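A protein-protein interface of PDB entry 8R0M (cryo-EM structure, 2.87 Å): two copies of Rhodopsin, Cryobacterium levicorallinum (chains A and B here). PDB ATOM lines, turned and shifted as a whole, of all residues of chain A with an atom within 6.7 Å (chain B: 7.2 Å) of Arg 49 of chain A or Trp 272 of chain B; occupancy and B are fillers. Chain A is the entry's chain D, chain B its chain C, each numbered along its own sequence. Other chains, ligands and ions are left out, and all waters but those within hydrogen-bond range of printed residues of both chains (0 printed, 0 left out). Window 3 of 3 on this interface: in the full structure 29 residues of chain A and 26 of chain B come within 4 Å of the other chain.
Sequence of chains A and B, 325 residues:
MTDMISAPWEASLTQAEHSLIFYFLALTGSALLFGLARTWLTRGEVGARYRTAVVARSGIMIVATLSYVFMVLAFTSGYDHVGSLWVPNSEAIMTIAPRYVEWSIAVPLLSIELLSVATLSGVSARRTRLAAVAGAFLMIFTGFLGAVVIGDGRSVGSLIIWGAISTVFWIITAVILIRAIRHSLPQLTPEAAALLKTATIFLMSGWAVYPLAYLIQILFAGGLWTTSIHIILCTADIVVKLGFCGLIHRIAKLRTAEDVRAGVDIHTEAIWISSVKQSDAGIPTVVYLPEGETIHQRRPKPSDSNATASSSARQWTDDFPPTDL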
ATOM      1  N   VAL A  46     -32.657  -5.623 -11.699  1.00  0.00           N
ATOM      2  CA  VAL A  46     -31.488  -5.849 -10.882  1.00  0.00           C
ATOM      3  C   VAL A  46     -30.745  -4.527 -10.706  1.00  0.00           C
ATOM      4  O   VAL A  46     -30.706  -3.689 -11.618  1.00  0.00           O
ATOM      5  CB  VAL A  46     -30.638  -6.929 -11.567  1.00  0.00           C
ATOM      6  CG1 VAL A  46     -29.248  -7.088 -10.978  1.00  0.00           C
ATOM      7  CG2 VAL A  46     -31.390  -8.252 -11.501  1.00  0.00           C
ATOM      8  N   GLY A  47     -30.129  -4.370  -9.530  1.00  0.00           N
ATOM      9  CA  GLY A  47     -29.300  -3.220  -9.246  1.00  0.00           C
ATOM     10  C   GLY A  47     -28.072  -3.180 -10.139  1.00  0.00           C
ATOM     11  O   GLY A  47     -27.696  -4.169 -10.723  1.00  0.00           O
ATOM     12  N   ALA A  48     -27.430  -2.029 -10.247  1.00  0.00           N
ATOM     13  CA  ALA A  48     -26.133  -1.935 -10.880  1.00  0.00           C
ATOM     14  C   ALA A  48     -25.058  -2.615 -10.044  1.00  0.00           C
ATOM     15  O   ALA A  48     -23.988  -2.889 -10.550  1.00  0.00           O
ATOM     16  CB  ALA A  48     -25.799  -0.486 -11.013  1.00  0.00           C
ATOM     17  N   ARG A  49     -25.287  -2.835  -8.763  1.00  0.00           N
ATOM     18  CA  ARG A  49     -24.317  -3.560  -7.979  1.00  0.00           C
ATOM     19  C   ARG A  49     -24.256  -5.001  -8.429  1.00  0.00           C
ATOM     20  O   ARG A  49     -23.258  -5.633  -8.134  1.00  0.00           O
ATOM     21  CB  ARG A  49     -24.724  -3.545  -6.521  1.00  0.00           C
ATOM     22  CG  ARG A  49     -23.750  -4.246  -5.626  1.00  0.00           C
ATOM     23  CD  ARG A  49     -24.160  -3.876  -4.237  1.00  0.00           C
ATOM     24  NE  ARG A  49     -23.246  -4.477  -3.314  1.00  0.00           N
ATOM     25  CZ  ARG A  49     -23.311  -4.327  -2.019  1.00  0.00           C
ATOM     26  NH1 ARG A  49     -24.401  -3.849  -1.455  1.00  0.00           N
ATOM     27  NH2 ARG A  49     -22.262  -4.659  -1.285  1.00  0.00           N
ATOM     28  N   TYR A  50     -25.306  -5.509  -9.084  1.00  0.00           N
ATOM     29  CA  TYR A  50     -25.449  -6.934  -9.297  1.00  0.00           C
ATOM     30  C   TYR A  50     -25.579  -7.204 -10.775  1.00  0.00           C
ATOM     31  O   TYR A  50     -26.015  -8.284 -11.134  1.00  0.00           O
ATOM     32  CB  TYR A  50     -26.655  -7.531  -8.570  1.00  0.00           C
ATOM     33  CG  TYR A  50     -26.527  -7.340  -7.080  1.00  0.00           C
ATOM     34  CD1 TYR A  50     -25.544  -7.965  -6.364  1.00  0.00           C
ATOM     35  CD2 TYR A  50     -27.360  -6.498  -6.404  1.00  0.00           C
ATOM     36  CE1 TYR A  50     -25.400  -7.772  -5.005  1.00  0.00           C
ATOM     37  CE2 TYR A  50     -27.230  -6.269  -5.045  1.00  0.00           C
ATOM     38  CZ  TYR A  50     -26.219  -6.888  -4.342  1.00  0.00           C
ATOM     39  OH  TYR A  50     -26.011  -6.664  -3.000  1.00  0.00           O
ATOM     40  N   ARG A  51     -25.150  -6.260 -11.608  1.00  0.00           N
ATOM     41  CA  ARG A  51     -25.399  -6.369 -13.025  1.00  0.00           C
ATOM     42  C   ARG A  51     -24.461  -7.405 -13.657  1.00  0.00           C
ATOM     43  O   ARG A  51     -24.710  -7.882 -14.761  1.00  0.00           O
ATOM     44  CB  ARG A  51     -25.291  -4.973 -13.626  1.00  0.00           C
ATOM     45  CG  ARG A  51     -25.299  -4.965 -15.151  1.00  0.00           C
ATOM     46  CD  ARG A  51     -25.402  -3.586 -15.793  1.00  0.00           C
ATOM     47  NE  ARG A  51     -26.549  -2.857 -15.252  1.00  0.00           N
ATOM     48  CZ  ARG A  51     -26.472  -1.654 -14.709  1.00  0.00           C
ATOM     49  NH1 ARG A  51     -25.350  -0.967 -14.788  1.00  0.00           N
ATOM     50  NH2 ARG A  51     -27.520  -1.129 -14.107  1.00  0.00           N
ATOM     51  N   THR A  52     -23.378  -7.778 -12.980  1.00  0.00           N
ATOM     52  CA  THR A  52     -22.475  -8.758 -13.541  1.00  0.00           C
ATOM     53  C   THR A  52     -23.251 -10.031 -13.814  1.00  0.00           C
ATOM     54  O   THR A  52     -22.922 -10.754 -14.749  1.00  0.00           O
ATOM     55  CB  THR A  52     -21.320  -9.078 -12.586  1.00  0.00           C
ATOM     56  OG1 THR A  52     -20.650  -7.841 -12.300  1.00  0.00           O
ATOM     57  CG2 THR A  52     -20.367 -10.135 -13.121  1.00  0.00           C
ATOM     58  N   SER A 116     -21.088 -13.697  -8.791  1.00  0.00           N
ATOM     59  CA  SER A 116     -21.755 -12.414  -8.933  1.00  0.00           C
ATOM     60  C   SER A 116     -22.571 -12.050  -7.698  1.00  0.00           C
ATOM     61  O   SER A 116     -22.445 -10.938  -7.197  1.00  0.00           O
ATOM     62  CB  SER A 116     -22.644 -12.467 -10.137  1.00  0.00           C
ATOM     63  OG  SER A 116     -23.326 -11.250 -10.325  1.00  0.00           O
ATOM     64  N   SER A 121     -15.602  -9.332  -2.363  1.00  0.00           N
ATOM     65  CA  SER A 121     -15.442  -7.999  -2.924  1.00  0.00           C
ATOM     66  C   SER A 121     -13.976  -7.591  -2.986  1.00  0.00           C
ATOM     67  O   SER A 121     -13.162  -8.042  -2.181  1.00  0.00           O
ATOM     68  CB  SER A 121     -16.271  -6.995  -2.177  1.00  0.00           C
ATOM     69  OG  SER A 121     -15.840  -6.884  -0.830  1.00  0.00           O
ATOM     70  N   ARG A 255     -31.456  -9.365  -3.588  1.00  0.00           N
ATOM     71  CA  ARG A 255     -30.360  -8.657  -2.952  1.00  0.00           C
ATOM     72  C   ARG A 255     -30.486  -7.183  -3.289  1.00  0.00           C
ATOM     73  O   ARG A 255     -30.077  -6.339  -2.502  1.00  0.00           O
ATOM     74  CB  ARG A 255     -29.012  -9.152  -3.500  1.00  0.00           C
ATOM     75  CG  ARG A 255     -28.653 -10.554  -3.069  1.00  0.00           C
ATOM     76  CD  ARG A 255     -27.638 -10.472  -1.992  1.00  0.00           C
ATOM     77  NE  ARG A 255     -26.335 -10.279  -2.575  1.00  0.00           N
ATOM     78  CZ  ARG A 255     -25.313  -9.838  -1.869  1.00  0.00           C
ATOM     79  NH1 ARG A 255     -25.481  -9.508  -0.600  1.00  0.00           N
ATOM     80  NH2 ARG A 255     -24.135  -9.658  -2.426  1.00  0.00           N
ATOM     81  N   THR A 256     -30.921  -6.908  -4.517  1.00  0.00           N
ATOM     82  CA  THR A 256     -31.099  -5.543  -4.945  1.00  0.00           C
ATOM     83  C   THR A 256     -32.119  -4.867  -4.048  1.00  0.00           C
ATOM     84  O   THR A 256     -31.904  -3.795  -3.530  1.00  0.00           O
ATOM     85  CB  THR A 256     -31.613  -5.492  -6.367  1.00  0.00           C
ATOM     86  OG1 THR A 256     -30.565  -5.943  -7.216  1.00  0.00           O
ATOM     87  CG2 THR A 256     -32.083  -4.123  -6.764  1.00  0.00           C
ATOM     88  N   ASP A 259     -31.111  -4.057  -0.562  1.00  0.00           N
ATOM     89  CA  ASP A 259     -30.218  -2.917  -0.459  1.00  0.00           C
ATOM     90  C   ASP A 259     -31.029  -1.650  -0.520  1.00  0.00           C
ATOM     91  O   ASP A 259     -30.774  -0.736   0.233  1.00  0.00           O
ATOM     92  CB  ASP A 259     -29.224  -2.795  -1.615  1.00  0.00           C
ATOM     93  CG  ASP A 259     -28.054  -3.780  -1.575  1.00  0.00           C
ATOM     94  OD1 ASP A 259     -27.807  -4.392  -0.493  1.00  0.00           O
ATOM     95  OD2 ASP A 259     -27.416  -3.958  -2.644  1.00  0.00           O
ATOM     96  N   VAL A 264     -28.663   1.342   1.017  1.00  0.00           N
ATOM     97  CA  VAL A 264     -27.487   1.147   0.199  1.00  0.00           C
ATOM     98  C   VAL A 264     -27.698   1.710  -1.209  1.00  0.00           C
ATOM     99  O   VAL A 264     -26.720   2.040  -1.858  1.00  0.00           O
ATOM    100  CB  VAL A 264     -27.129  -0.347   0.189  1.00  0.00           C
ATOM    101  CG1 VAL A 264     -26.047  -0.730  -0.820  1.00  0.00           C
ATOM    102  CG2 VAL A 264     -26.739  -0.773   1.583  1.00  0.00           C
ATOM    103  N   ASP A 265     -28.922   1.750  -1.733  1.00  0.00           N
ATOM    104  CA  ASP A 265     -29.087   2.203  -3.103  1.00  0.00           C
ATOM    105  C   ASP A 265     -30.560   2.423  -3.397  1.00  0.00           C
ATOM    106  O   ASP A 265     -31.364   2.378  -2.480  1.00  0.00           O
ATOM    107  CB  ASP A 265     -28.443   1.226  -4.077  1.00  0.00           C
ATOM    108  CG  ASP A 265     -27.800   1.838  -5.319  1.00  0.00           C
ATOM    109  OD1 ASP A 265     -28.142   3.025  -5.677  1.00  0.00           O
ATOM    110  OD2 ASP A 265     -26.931   1.118  -5.933  1.00  0.00           O
ATOM    111  N   GLU B  45     -23.251   3.072 -17.420  1.00  0.00           N
ATOM    112  CA  GLU B  45     -22.457   3.102 -16.174  1.00  0.00           C
ATOM    113  C   GLU B  45     -21.391   4.172 -16.344  1.00  0.00           C
ATOM    114  O   GLU B  45     -20.766   4.524 -15.368  1.00  0.00           O
ATOM    115  CB  GLU B  45     -21.836   1.729 -15.983  1.00  0.00           C
ATOM    116  CG  GLU B  45     -22.837   0.618 -15.840  1.00  0.00           C
ATOM    117  CD  GLU B  45     -22.172  -0.723 -15.617  1.00  0.00           C
ATOM    118  OE1 GLU B  45     -22.881  -1.686 -15.313  1.00  0.00           O
ATOM    119  OE2 GLU B  45     -20.949  -0.790 -15.757  1.00  0.00           O
ATOM    120  N   LYS B 253     -15.634   4.637 -15.755  1.00  0.00           N
ATOM    121  CA  LYS B 253     -16.560   4.615 -14.638  1.00  0.00           C
ATOM    122  C   LYS B 253     -15.944   5.330 -13.468  1.00  0.00           C
ATOM    123  O   LYS B 253     -16.568   6.084 -12.766  1.00  0.00           O
ATOM    124  CB  LYS B 253     -16.898   3.200 -14.209  1.00  0.00           C
ATOM    125  CG  LYS B 253     -17.733   2.476 -15.257  1.00  0.00           C
ATOM    126  CD  LYS B 253     -18.002   1.048 -14.896  1.00  0.00           C
ATOM    127  CE  LYS B 253     -18.495   0.911 -13.470  1.00  0.00           C
ATOM    128  NZ  LYS B 253     -18.874  -0.493 -13.223  1.00  0.00           N
ATOM    129  N   ALA B 257     -17.604   8.743 -11.928  1.00  0.00           N
ATOM    130  CA  ALA B 257     -17.932   8.856 -10.529  1.00  0.00           C
ATOM    131  C   ALA B 257     -17.163   9.991  -9.889  1.00  0.00           C
ATOM    132  O   ALA B 257     -17.679  10.637  -8.999  1.00  0.00           O
ATOM    133  CB  ALA B 257     -17.628   7.553  -9.846  1.00  0.00           C
ATOM    134  N   GLU B 269     -27.582   6.418 -12.414  1.00  0.00           N
ATOM    135  CA  GLU B 269     -27.372   5.268 -11.555  1.00  0.00           C
ATOM    136  C   GLU B 269     -26.225   5.590 -10.604  1.00  0.00           C
ATOM    137  O   GLU B 269     -25.454   6.501 -10.879  1.00  0.00           O
ATOM    138  CB  GLU B 269     -26.907   4.010 -12.297  1.00  0.00           C
ATOM    139  CG  GLU B 269     -27.586   3.623 -13.594  1.00  0.00           C
ATOM    140  CD  GLU B 269     -26.856   2.466 -14.285  1.00  0.00           C
ATOM    141  OE1 GLU B 269     -27.267   2.054 -15.417  1.00  0.00           O
ATOM    142  OE2 GLU B 269     -25.863   1.971 -13.691  1.00  0.00           O
ATOM    143  N   ALA B 270     -26.039   4.757  -9.571  1.00  0.00           N
ATOM    144  CA  ALA B 270     -24.782   4.716  -8.847  1.00  0.00           C
ATOM    145  C   ALA B 270     -23.720   3.905  -9.587  1.00  0.00           C
ATOM    146  O   ALA B 270     -24.038   3.000 -10.347  1.00  0.00           O
ATOM    147  CB  ALA B 270     -24.974   4.097  -7.516  1.00  0.00           C
ATOM    148  N   ILE B 271     -22.455   4.234  -9.310  1.00  0.00           N
ATOM    149  CA  ILE B 271     -21.348   3.534  -9.890  1.00  0.00           C
ATOM    150  C   ILE B 271     -20.806   2.630  -8.800  1.00  0.00           C
ATOM    151  O   ILE B 271     -20.485   3.091  -7.709  1.00  0.00           O
ATOM    152  CB  ILE B 271     -20.289   4.492 -10.457  1.00  0.00           C
ATOM    153  CG1 ILE B 271     -20.709   5.098 -11.785  1.00  0.00           C
ATOM    154  CG2 ILE B 271     -18.963   3.772 -10.693  1.00  0.00           C
ATOM    155  CD1 ILE B 271     -21.455   6.348 -11.652  1.00  0.00           C
ATOM    156  N   TRP B 272     -20.812   1.331  -9.067  1.00  0.00           N
ATOM    157  CA  TRP B 272     -20.247   0.335  -8.157  1.00  0.00           C
ATOM    158  C   TRP B 272     -19.091  -0.221  -8.922  1.00  0.00           C
ATOM    159  O   TRP B 272     -19.313  -0.574 -10.048  1.00  0.00           O
ATOM    160  CB  TRP B 272     -21.297  -0.735  -7.849  1.00  0.00           C
ATOM    161  CG  TRP B 272     -22.474  -0.294  -7.033  1.00  0.00           C
ATOM    162  CD1 TRP B 272     -23.620   0.296  -7.468  1.00  0.00           C
ATOM    163  CD2 TRP B 272     -22.604  -0.436  -5.611  1.00  0.00           C
ATOM    164  NE1 TRP B 272     -24.455   0.535  -6.415  1.00  0.00           N
ATOM    165  CE2 TRP B 272     -23.859   0.095  -5.264  1.00  0.00           C
ATOM    166  CE3 TRP B 272     -21.788  -0.960  -4.609  1.00  0.00           C
ATOM    167  CZ2 TRP B 272     -24.312   0.116  -3.950  1.00  0.00           C
ATOM    168  CZ3 TRP B 272     -22.234  -0.926  -3.311  1.00  0.00           C
ATOM    169  CH2 TRP B 272     -23.478  -0.400  -2.990  1.00  0.00           C
ATOM    170  N   ILE B 273     -17.888  -0.103  -8.415  1.00  0.00           N
ATOM    171  CA  ILE B 273     -16.713  -0.707  -9.081  1.00  0.00           C
ATOM    172  C   ILE B 273     -16.130  -1.663  -8.064  1.00  0.00           C
ATOM    173  O   ILE B 273     -15.622  -1.161  -7.088  1.00  0.00           O
ATOM    174  CB  ILE B 273     -15.655   0.333  -9.498  1.00  0.00           C
ATOM    175  CG1 ILE B 273     -16.180   1.363 -10.494  1.00  0.00           C
ATOM    176  CG2 ILE B 273     -14.410  -0.352 -10.025  1.00  0.00           C
ATOM    177  CD1 ILE B 273     -15.124   2.325 -10.918  1.00  0.00           C
ATOM    178  N   SER B 274     -16.006  -2.943  -8.386  1.00  0.00           N
ATOM    179  CA  SER B 274     -15.567  -3.968  -7.412  1.00  0.00           C
ATOM    180  C   SER B 274     -16.532  -4.067  -6.239  1.00  0.00           C
ATOM    181  O   SER B 274     -16.073  -4.118  -5.113  1.00  0.00           O
ATOM    182  CB  SER B 274     -14.182  -3.673  -6.953  1.00  0.00           C
ATOM    183  OG  SER B 274     -13.239  -3.908  -7.987  1.00  0.00           O
ATOM    184  N   SER B 275     -17.824  -4.077  -6.504  1.00  0.00           N
ATOM    185  CA  SER B 275     -18.863  -4.087  -5.445  1.00  0.00           C
ATOM    186  C   SER B 275     -18.559  -3.007  -4.427  1.00  0.00           C
ATOM    187  O   SER B 275     -19.001  -3.157  -3.301  1.00  0.00           O
ATOM    188  CB  SER B 275     -19.025  -5.417  -4.817  1.00  0.00           C
ATOM    189  OG  SER B 275     -20.310  -5.949  -5.100  1.00  0.00           O
ATOM    190  N   VAL B 276     -17.818  -1.973  -4.821  1.00  0.00           N
ATOM    191  CA  VAL B 276     -17.668  -0.830  -3.932  1.00  0.00           C
ATOM    192  C   VAL B 276     -18.319   0.398  -4.551  1.00  0.00           C
ATOM    193  O   VAL B 276     -18.038   0.725  -5.700  1.00  0.00           O
ATOM    194  CB  VAL B 276     -16.194  -0.551  -3.661  1.00  0.00           C
ATOM    195  CG1 VAL B 276     -15.993   0.735  -2.903  1.00  0.00           C
ATOM    196  CG2 VAL B 276     -15.601  -1.708  -2.904  1.00  0.00           C
ATOM    197  N   LYS B 277     -19.186   1.076  -3.798  1.00  0.00           N
ATOM    198  CA  LYS B 277     -19.945   2.159  -4.384  1.00  0.00           C
ATOM    199  C   LYS B 277     -19.052   3.381  -4.472  1.00  0.00           C
ATOM    200  O   LYS B 277     -18.435   3.748  -3.475  1.00  0.00           O
ATOM    201  CB  LYS B 277     -21.190   2.501  -3.585  1.00  0.00           C
ATOM    202  CG  LYS B 277     -22.265   3.101  -4.465  1.00  0.00           C
ATOM    203  CD  LYS B 277     -23.094   4.111  -3.805  1.00  0.00           C
ATOM    204  CE  LYS B 277     -24.113   3.461  -2.933  1.00  0.00           C
ATOM    205  NZ  LYS B 277     -25.105   4.479  -2.503  1.00  0.00           N
ATOM    206  N   GLN B 278     -18.939   3.926  -5.695  1.00  0.00           N
ATOM    207  CA  GLN B 278     -18.056   5.029  -6.003  1.00  0.00           C
ATOM    208  C   GLN B 278     -18.847   6.305  -5.890  1.00  0.00           C
ATOM    209  O   GLN B 278     -18.333   7.261  -5.341  1.00  0.00           O
ATOM    210  CB  GLN B 278     -17.503   4.878  -7.420  1.00  0.00           C
ATOM    211  CG  GLN B 278     -16.696   3.599  -7.636  1.00  0.00           C
ATOM    212  CD  GLN B 278     -15.546   3.495  -6.666  1.00  0.00           C
ATOM    213  OE1 GLN B 278     -15.004   4.505  -6.207  1.00  0.00           O
ATOM    214  NE2 GLN B 278     -15.181   2.259  -6.334  1.00  0.00           N
ATOM    215  N   SER B 279     -20.095   6.290  -6.372  1.00  0.00           N
ATOM    216  CA  SER B 279     -20.951   7.473  -6.417  1.00  0.00           C
ATOM    217  C   SER B 279     -22.415   7.073  -6.322  1.00  0.00           C
ATOM    218  O   SER B 279     -22.782   6.018  -6.818  1.00  0.00           O
ATOM    219  CB  SER B 279     -20.753   8.269  -7.698  1.00  0.00           C
ATOM    220  OG  SER B 279     -21.359   7.616  -8.816  1.00  0.00           O
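NZ of Lys 277 of chain B sits at hydrogen-bond distance from O of Val 264 of chain A.
The side-chain carboxylate (OE1) of Glu 45 of chain B lies within salt-bridge range of the guanidinium group (NH1) of Arg 51 of chain A (2.6 Å).
The guanidinium group (NH1) of Arg 51 of chain A is in salt-bridge range of the side-chain carboxylate (OE2) of Glu 269 of chain B (3.2 Å).
NE1 of Trp 272 of chain B sits at hydrogen-bond distance from OD2 of Asp 265 of chain A (2.6 Å).
The guanidinium group of Arg 49 of chain A lies within salt-bridge range of the side-chain carboxylate of Asp 259 of chain A, at 3.2 Å.
The side-chain amino group of Lys 253 of chain B is in salt-bridge range of the side-chain carboxylate of Glu 45 of chain B, 3.3 Å away.
O of Trp 272 of chain B is in hydrogen-bond range of NZ of Lys 253 of chain B (3.2 Å).
The backbone carbonyl oxygen of Asp 259 of chain A sits at hydrogen-bond distance from the backbone NH of Val 264 of chain A (3.1 Å).
Among the printed residues, merely in contact across the chains: Ala 48 of chain A with Glu 269 of chain B, Ala 48 of chain A with Ala 270 of chain B, Arg 49 of chain A with Trp 272 of chain B, Arg 49 of chain A with Ser 275 of chain B, Val 264 of chain A with Trp 272 of chain B and Asp 265 of chain A with Ala 270 of chain B.
Arg 49 of chain A touches just these residues of chain B: Trp 272 and Ser 275.
Of the printed residues of chain B, Arg 51 of chain A touches Glu 45 and Glu 269.
Printed residues of chain B within 4 Å of Val 264 of chain A: Trp 272 (3.4 Å) and Lys 277 (3.0 Å).
Of the printed residues of chain B, Asp 265 of chain A touches Ala 270 (3.8 Å) and Trp 272 (2.6 Å).
Of the printed residues of chain A, Trp 272 of chain B touches Arg 49 (3.6 Å), Val 264 (3.4 Å) and Asp 265 (2.6 Å).
Val 276 of chain B touches none of the printed residues of chain A.
Of the printed residues of chain A, Lys 277 of chain B touches Val 264 (3.0 Å).
Ser 279 of chain B touches none of the printed residues of chain A.
The nearest printed residue of chain B that does not touch Arg 49 of chain A is Val 276 of chain B (6.2 Å).
Of the 14 printed residues of chain A, 5 touch a printed residue of chain B.
Among the printed residues, 10 pairs touch across the chains.
Among the printed residues, Asp or Glu carboxylates within 4 Å of a Lys or Arg side-chain nitrogen of the other chain: Arg 51 of chain A with Glu 45 of chain B (2.6 Å) and Arg 51 of chain A with Glu 269 of chain B (3.2 Å).
No position is printed for both chains.
Of the 10 pairs that touch across the chains among the printed residues, none has its exchanged pair printed and touching as well.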
